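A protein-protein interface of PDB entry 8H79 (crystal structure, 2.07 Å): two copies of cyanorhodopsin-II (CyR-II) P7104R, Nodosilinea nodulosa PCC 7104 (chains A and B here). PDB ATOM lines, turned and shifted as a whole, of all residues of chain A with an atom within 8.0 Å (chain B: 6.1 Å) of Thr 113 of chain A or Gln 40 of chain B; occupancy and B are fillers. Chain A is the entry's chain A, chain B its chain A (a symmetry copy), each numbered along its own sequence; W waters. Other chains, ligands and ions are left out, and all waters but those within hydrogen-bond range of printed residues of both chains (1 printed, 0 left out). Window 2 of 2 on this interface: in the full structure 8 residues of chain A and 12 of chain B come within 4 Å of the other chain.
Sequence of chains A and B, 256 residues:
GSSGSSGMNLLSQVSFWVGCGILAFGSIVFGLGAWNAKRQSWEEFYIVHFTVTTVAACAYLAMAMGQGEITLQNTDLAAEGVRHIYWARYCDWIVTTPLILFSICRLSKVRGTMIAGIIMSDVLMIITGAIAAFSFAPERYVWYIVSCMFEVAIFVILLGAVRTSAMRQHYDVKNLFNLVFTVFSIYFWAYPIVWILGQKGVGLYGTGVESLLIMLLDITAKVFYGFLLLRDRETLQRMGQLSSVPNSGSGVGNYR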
ATOM      1  N   VAL A 110       3.503  13.118   2.059  1.00  0.00           N
ATOM      2  CA  VAL A 110       4.067  13.539   3.339  1.00  0.00           C
ATOM      3  C   VAL A 110       3.858  15.038   3.530  1.00  0.00           C
ATOM      4  O   VAL A 110       3.716  15.802   2.565  1.00  0.00           O
ATOM      5  CB  VAL A 110       5.560  13.150   3.423  1.00  0.00           C
ATOM      6  CG1 VAL A 110       6.418  14.046   2.517  1.00  0.00           C
ATOM      7  CG2 VAL A 110       6.064  13.188   4.873  1.00  0.00           C
ATOM      8  N   ARG A 111       3.822  15.460   4.793  1.00  0.00           N
ATOM      9  CA  ARG A 111       3.629  16.861   5.126  1.00  0.00           C
ATOM     10  C   ARG A 111       4.774  17.711   4.572  1.00  0.00           C
ATOM     11  O   ARG A 111       5.895  17.240   4.376  1.00  0.00           O
ATOM     12  CB  ARG A 111       3.534  17.036   6.643  1.00  0.00           C
ATOM     13  CG  ARG A 111       4.732  16.476   7.405  1.00  0.00           C
ATOM     14  CD  ARG A 111       4.466  16.430   8.906  1.00  0.00           C
ATOM     15  NE  ARG A 111       5.594  15.905   9.667  1.00  0.00           N
ATOM     16  CZ  ARG A 111       5.879  14.617   9.797  1.00  0.00           C
ATOM     17  NH1 ARG A 111       5.162  13.685   9.192  1.00  0.00           N
ATOM     18  NH2 ARG A 111       6.909  14.255  10.554  1.00  0.00           N
ATOM     19  N   GLY A 112       4.476  18.997   4.352  1.00  0.00           N
ATOM     20  CA  GLY A 112       5.415  19.882   3.678  1.00  0.00           C
ATOM     21  C   GLY A 112       6.711  20.137   4.428  1.00  0.00           C
ATOM     22  O   GLY A 112       7.739  20.425   3.810  1.00  0.00           O
ATOM     23  N   THR A 113       6.689  20.060   5.760  1.00  0.00           N
ATOM     24  CA  THR A 113       7.909  20.308   6.520  1.00  0.00           C
ATOM     25  C   THR A 113       8.980  19.276   6.204  1.00  0.00           C
ATOM     26  O   THR A 113      10.174  19.593   6.214  1.00  0.00           O
ATOM     27  CB  THR A 113       7.615  20.298   8.016  1.00  0.00           C
ATOM     28  OG1 THR A 113       6.817  19.150   8.328  1.00  0.00           O
ATOM     29  CG2 THR A 113       6.868  21.568   8.424  1.00  0.00           C
ATOM     30  N   MET A 114       8.572  18.035   5.937  1.00  0.00           N
ATOM     31  CA  MET A 114       9.531  16.999   5.586  1.00  0.00           C
ATOM     32  C   MET A 114      10.081  17.225   4.184  1.00  0.00           C
ATOM     33  O   MET A 114      11.266  16.980   3.930  1.00  0.00           O
ATOM     34  CB  MET A 114       8.868  15.630   5.705  1.00  0.00           C
ATOM     35  CG  MET A 114       8.555  15.220   7.146  1.00  0.00           C
ATOM     36  SD  MET A 114       9.990  15.205   8.242  1.00  0.00           S
ATOM     37  CE  MET A 114       9.721  16.668   9.250  1.00  0.00           C
ATOM     38  N   ILE A 115       9.234  17.704   3.268  1.00  0.00           N
ATOM     39  CA  ILE A 115       9.692  18.047   1.921  1.00  0.00           C
ATOM     40  C   ILE A 115      10.759  19.132   1.987  1.00  0.00           C
ATOM     41  O   ILE A 115      11.802  19.043   1.327  1.00  0.00           O
ATOM     42  CB  ILE A 115       8.503  18.481   1.040  1.00  0.00           C
ATOM     43  CG1 ILE A 115       7.548  17.315   0.791  1.00  0.00           C
ATOM     44  CG2 ILE A 115       8.989  19.060  -0.294  1.00  0.00           C
ATOM     45  CD1 ILE A 115       6.442  17.635  -0.233  1.00  0.00           C
ATOM     46  N   ALA A 116      10.503  20.182   2.774  1.00  0.00           N
ATOM     47  CA  ALA A 116      11.466  21.270   2.908  1.00  0.00           C
ATOM     48  C   ALA A 116      12.765  20.788   3.541  1.00  0.00           C
ATOM     49  O   ALA A 116      13.855  21.204   3.134  1.00  0.00           O
ATOM     50  CB  ALA A 116      10.860  22.409   3.727  1.00  0.00           C
ATOM     51  N   GLY A 117      12.670  19.905   4.538  1.00  0.00           N
ATOM     52  CA  GLY A 117      13.876  19.403   5.173  1.00  0.00           C
ATOM     53  C   GLY A 117      14.707  18.534   4.249  1.00  0.00           C
ATOM     54  O   GLY A 117      15.938  18.630   4.230  1.00  0.00           O
ATOM     55  N   ILE A 118      14.053  17.673   3.469  1.00  0.00           N
ATOM     56  CA  ILE A 118      14.806  16.771   2.607  1.00  0.00           C
ATOM     57  C   ILE A 118      15.413  17.527   1.425  1.00  0.00           C
ATOM     58  O   ILE A 118      16.523  17.215   0.984  1.00  0.00           O
ATOM     59  CB  ILE A 118      13.920  15.589   2.161  1.00  0.00           C
ATOM     60  CG1 ILE A 118      14.778  14.336   1.956  1.00  0.00           C
ATOM     61  CG2 ILE A 118      13.140  15.922   0.901  1.00  0.00           C
ATOM     62  CD1 ILE A 118      13.969  13.045   1.782  1.00  0.00           C
ATOM     63  N   ILE A 119      14.724  18.555   0.916  1.00  0.00           N
ATOM     64  CA  ILE A 119      15.294  19.355  -0.169  1.00  0.00           C
ATOM     65  C   ILE A 119      16.518  20.126   0.320  1.00  0.00           C
ATOM     66  O   ILE A 119      17.540  20.205  -0.377  1.00  0.00           O
ATOM     67  CB  ILE A 119      14.224  20.294  -0.759  1.00  0.00           C
ATOM     68  CG1 ILE A 119      13.187  19.491  -1.545  1.00  0.00           C
ATOM     69  CG2 ILE A 119      14.863  21.364  -1.662  1.00  0.00           C
ATOM     70  CD1 ILE A 119      12.080  20.335  -2.153  1.00  0.00           C
ATOM     71  N   MET A 120      16.442  20.692   1.532  1.00  0.00           N
ATOM     72  CA  MET A 120      17.569  21.442   2.084  1.00  0.00           C
ATOM     73  C   MET A 120      18.793  20.550   2.252  1.00  0.00           C
ATOM     74  O   MET A 120      19.904  20.923   1.858  1.00  0.00           O
ATOM     75  CB  MET A 120      17.189  22.070   3.426  1.00  0.00           C
ATOM     76  CG  MET A 120      18.393  22.686   4.144  1.00  0.00           C
ATOM     77  SD  MET A 120      19.181  21.590   5.346  1.00  0.00           S
ATOM     78  CE  MET A 120      17.795  21.192   6.417  1.00  0.00           C
ATOM     79  N   ILE A 157      15.321  11.259   7.026  1.00  0.00           N
ATOM     80  CA  ILE A 157      14.008  11.810   6.713  1.00  0.00           C
ATOM     81  C   ILE A 157      13.227  10.866   5.808  1.00  0.00           C
ATOM     82  O   ILE A 157      12.025  10.649   6.006  1.00  0.00           O
ATOM     83  CB  ILE A 157      14.153  13.201   6.074  1.00  0.00           C
ATOM     84  CG1 ILE A 157      14.948  14.143   6.980  1.00  0.00           C
ATOM     85  CG2 ILE A 157      12.778  13.791   5.762  1.00  0.00           C
ATOM     86  CD1 ILE A 157      15.253  15.480   6.330  1.00  0.00           C
ATOM     87  N   ALA A 161      10.184   9.639   8.247  1.00  0.00           N
ATOM     88  CA  ALA A 161       8.867  10.268   8.153  1.00  0.00           C
ATOM     89  C   ALA A 161       8.207  10.043   6.793  1.00  0.00           C
ATOM     90  O   ALA A 161       6.992   9.822   6.727  1.00  0.00           O
ATOM     91  CB  ALA A 161       8.982  11.762   8.452  1.00  0.00           C
ATOM     92  N   LYS B  38       7.102  17.105  17.263  1.00  0.00           N
ATOM     93  CA  LYS B  38       5.894  16.409  16.841  1.00  0.00           C
ATOM     94  C   LYS B  38       4.922  17.313  16.092  1.00  0.00           C
ATOM     95  O   LYS B  38       4.253  16.856  15.161  1.00  0.00           O
ATOM     96  CB  LYS B  38       5.190  15.788  18.054  1.00  0.00           C
ATOM     97  CG  LYS B  38       6.119  15.031  19.003  1.00  0.00           C
ATOM     98  CD  LYS B  38       6.518  13.675  18.441  1.00  0.00           C
ATOM     99  CE  LYS B  38       7.462  12.943  19.394  1.00  0.00           C
ATOM    100  NZ  LYS B  38       7.576  11.482  19.093  1.00  0.00           N
ATOM    101  N   ARG B  39       4.839  18.587  16.467  1.00  0.00           N
ATOM    102  CA  ARG B  39       3.959  19.527  15.789  1.00  0.00           C
ATOM    103  C   ARG B  39       4.631  20.098  14.545  1.00  0.00           C
ATOM    104  O   ARG B  39       5.822  20.426  14.560  1.00  0.00           O
ATOM    105  CB  ARG B  39       3.566  20.664  16.730  1.00  0.00           C
ATOM    106  CG  ARG B  39       2.933  20.209  18.037  1.00  0.00           C
ATOM    107  CD  ARG B  39       1.965  21.253  18.580  1.00  0.00           C
ATOM    108  NE  ARG B  39       0.573  20.909  18.314  1.00  0.00           N
ATOM    109  CZ  ARG B  39      -0.102  21.279  17.234  1.00  0.00           C
ATOM    110  NH1 ARG B  39      -1.360  20.912  17.045  1.00  0.00           N
ATOM    111  NH2 ARG B  39       0.499  22.038  16.319  1.00  0.00           N
ATOM    112  N   GLN B  40       3.847  20.244  13.471  1.00  0.00           N
ATOM    113  CA  GLN B  40       4.390  20.736  12.209  1.00  0.00           C
ATOM    114  C   GLN B  40       5.017  22.118  12.360  1.00  0.00           C
ATOM    115  O   GLN B  40       6.043  22.411  11.732  1.00  0.00           O
ATOM    116  CB  GLN B  40       3.297  20.763  11.143  1.00  0.00           C
ATOM    117  CG  GLN B  40       3.759  20.256   9.796  1.00  0.00           C
ATOM    118  CD  GLN B  40       2.609  19.982   8.841  1.00  0.00           C
ATOM    119  OE1 GLN B  40       1.858  19.026   9.018  1.00  0.00           O
ATOM    120  NE2 GLN B  40       2.481  20.811   7.811  1.00  0.00           N
ATOM    121  N   SER B  41       4.421  22.982  13.186  1.00  0.00           N
ATOM    122  CA  SER B  41       4.924  24.350  13.295  1.00  0.00           C
ATOM    123  C   SER B  41       6.261  24.401  14.025  1.00  0.00           C
ATOM    124  O   SER B  41       7.043  25.339  13.822  1.00  0.00           O
ATOM    125  CB  SER B  41       3.890  25.234  13.994  1.00  0.00           C
ATOM    126  OG  SER B  41       3.959  25.086  15.398  1.00  0.00           O
ATOM    127  N   TRP B  42       6.539  23.409  14.874  1.00  0.00           N
ATOM    128  CA  TRP B  42       7.853  23.304  15.493  1.00  0.00           C
ATOM    129  C   TRP B  42       8.862  22.678  14.536  1.00  0.00           C
ATOM    130  O   TRP B  42      10.032  23.080  14.517  1.00  0.00           O
ATOM    131  CB  TRP B  42       7.753  22.493  16.789  1.00  0.00           C
ATOM    132  CG  TRP B  42       7.363  23.312  17.996  1.00  0.00           C
ATOM    133  CD1 TRP B  42       6.175  23.266  18.672  1.00  0.00           C
ATOM    134  CD2 TRP B  42       8.171  24.287  18.675  1.00  0.00           C
ATOM    135  NE1 TRP B  42       6.196  24.151  19.728  1.00  0.00           N
ATOM    136  CE2 TRP B  42       7.406  24.791  19.747  1.00  0.00           C
ATOM    137  CE3 TRP B  42       9.463  24.783  18.474  1.00  0.00           C
ATOM    138  CZ2 TRP B  42       7.890  25.767  20.613  1.00  0.00           C
ATOM    139  CZ3 TRP B  42       9.943  25.749  19.344  1.00  0.00           C
ATOM    140  CH2 TRP B  42       9.159  26.226  20.399  1.00  0.00           C
ATOM    141  N   GLU B  43       8.430  21.688  13.748  1.00  0.00           N
ATOM    142  CA  GLU B  43       9.283  21.140  12.698  1.00  0.00           C
ATOM    143  C   GLU B  43       9.754  22.237  11.752  1.00  0.00           C
ATOM    144  O   GLU B  43      10.941  22.316  11.422  1.00  0.00           O
ATOM    145  CB  GLU B  43       8.540  20.045  11.925  1.00  0.00           C
ATOM    146  CG  GLU B  43       8.420  18.718  12.670  1.00  0.00           C
ATOM    147  CD  GLU B  43       7.526  17.716  11.959  1.00  0.00           C
ATOM    148  OE1 GLU B  43       6.839  18.101  10.988  1.00  0.00           O
ATOM    149  OE2 GLU B  43       7.509  16.535  12.378  1.00  0.00           O
ATOM    150  N   GLU B  44       8.834  23.104  11.315  1.00  0.00           N
ATOM    151  CA  GLU B  44       9.218  24.192  10.419  1.00  0.00           C
ATOM    152  C   GLU B  44      10.193  25.148  11.091  1.00  0.00           C
ATOM    153  O   GLU B  44      11.193  25.554  10.483  1.00  0.00           O
ATOM    154  CB  GLU B  44       7.990  24.962   9.934  1.00  0.00           C
ATOM    155  CG  GLU B  44       8.359  26.269   9.210  1.00  0.00           C
ATOM    156  CD  GLU B  44       7.154  27.084   8.791  1.00  0.00           C
ATOM    157  OE1 GLU B  44       6.243  26.511   8.168  1.00  0.00           O
ATOM    158  OE2 GLU B  44       7.121  28.300   9.068  1.00  0.00           O
ATOM    159  N   PHE B  45       9.920  25.524  12.345  1.00  0.00           N
ATOM    160  CA  PHE B  45      10.807  26.453  13.044  1.00  0.00           C
ATOM    161  C   PHE B  45      12.224  25.899  13.124  1.00  0.00           C
ATOM    162  O   PHE B  45      13.198  26.587  12.792  1.00  0.00           O
ATOM    163  CB  PHE B  45      10.279  26.741  14.452  1.00  0.00           C
ATOM    164  CG  PHE B  45      11.240  27.529  15.295  1.00  0.00           C
ATOM    165  CD1 PHE B  45      11.326  28.905  15.154  1.00  0.00           C
ATOM    166  CD2 PHE B  45      12.072  26.895  16.199  1.00  0.00           C
ATOM    167  CE1 PHE B  45      12.221  29.648  15.926  1.00  0.00           C
ATOM    168  CE2 PHE B  45      12.973  27.625  16.967  1.00  0.00           C
ATOM    169  CZ  PHE B  45      13.048  29.003  16.824  1.00  0.00           C
ATOM    170  N   ILE B  47      13.641  23.439  11.372  1.00  0.00           N
ATOM    171  CA  ILE B  47      14.271  23.206  10.076  1.00  0.00           C
ATOM    172  C   ILE B  47      14.813  24.507   9.511  1.00  0.00           C
ATOM    173  O   ILE B  47      15.931  24.551   8.988  1.00  0.00           O
ATOM    174  CB  ILE B  47      13.279  22.541   9.104  1.00  0.00           C
ATOM    175  CG1 ILE B  47      13.131  21.057   9.425  1.00  0.00           C
ATOM    176  CG2 ILE B  47      13.736  22.719   7.658  1.00  0.00           C
ATOM    177  CD1 ILE B  47      11.939  20.430   8.737  1.00  0.00           C
HETATM  178  O   HOH W   1       1.798  20.254   4.931  1.00  0.00           O
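The guanidinium group (NE) of Arg 111 of chain A lies within salt-bridge range of the side-chain carboxylate (OE1) of Glu 43 of chain B (2.8 Å). The side-chain hydroxyl (OG1) of Thr 113 of chain A sits at hydrogen-bond distance from the side-chain carboxylate (OE1) of Glu 43 of chain B (2.9 Å).
Of the printed residues of chain B, Thr 113 of chain A touches Gln 40, Glu 43, Glu 44 and Ile 47. Gln 40 of chain B touches just these residues of chain A: Arg 111 (3.5 Å) and Thr 113 (3.5 Å). Of the printed residues of chain A, Ile 47 of chain B touches Thr 113 (3.2 Å). Printed residues of chain B within 4 Å of Arg 111 of chain A: Gln 40 and Glu 43. Printed residues of chain A within 4 Å of Glu 43 of chain B: Arg 111 (2.8 Å), Thr 113 (2.9 Å) and Met 114 (3.6 Å). Gly 112 of chain A touches none of the printed residues of chain B. The nearest residue of chain B that does not touch Thr 113 of chain A is Ser 41 of chain B (5.5 Å). The nearest residue of chain A that does not touch Gln 40 of chain B is Gly 112 of chain A (4.4 Å). The nearest printed residue of chain A that does not touch Glu 43 of chain B is Ala 161 of chain A (6.4 Å).
Among the printed residues, pairs that only touch across the chains: Arg 111 of chain A with Gln 40 of chain B (3.5 Å), Thr 113 of chain A with Gln 40 of chain B (3.5 Å), Thr 113 of chain A with Glu 44 of chain B (3.8 Å), Thr 113 of chain A with Ile 47 of chain B (3.2 Å) and Met 114 of chain A with Glu 43 of chain B (3.6 Å).
Water W1 bridges NE2 of Gln 40 of chain B (3.0 Å) and N of Gly 112 of chain A (3.0 Å).
Of the 9 printed residues of chain B, 4 touch a printed residue of chain A. Printed residues of chain B that touch a printed residue of chain A: Gln 40, Glu 43, Glu 44 and Ile 47. Among the printed residues, 7 pairs touch across the chains.
No position is printed for both chains. Of the 7 pairs that touch across the chains among the printed residues, none has its exchanged pair printed and touching as well.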
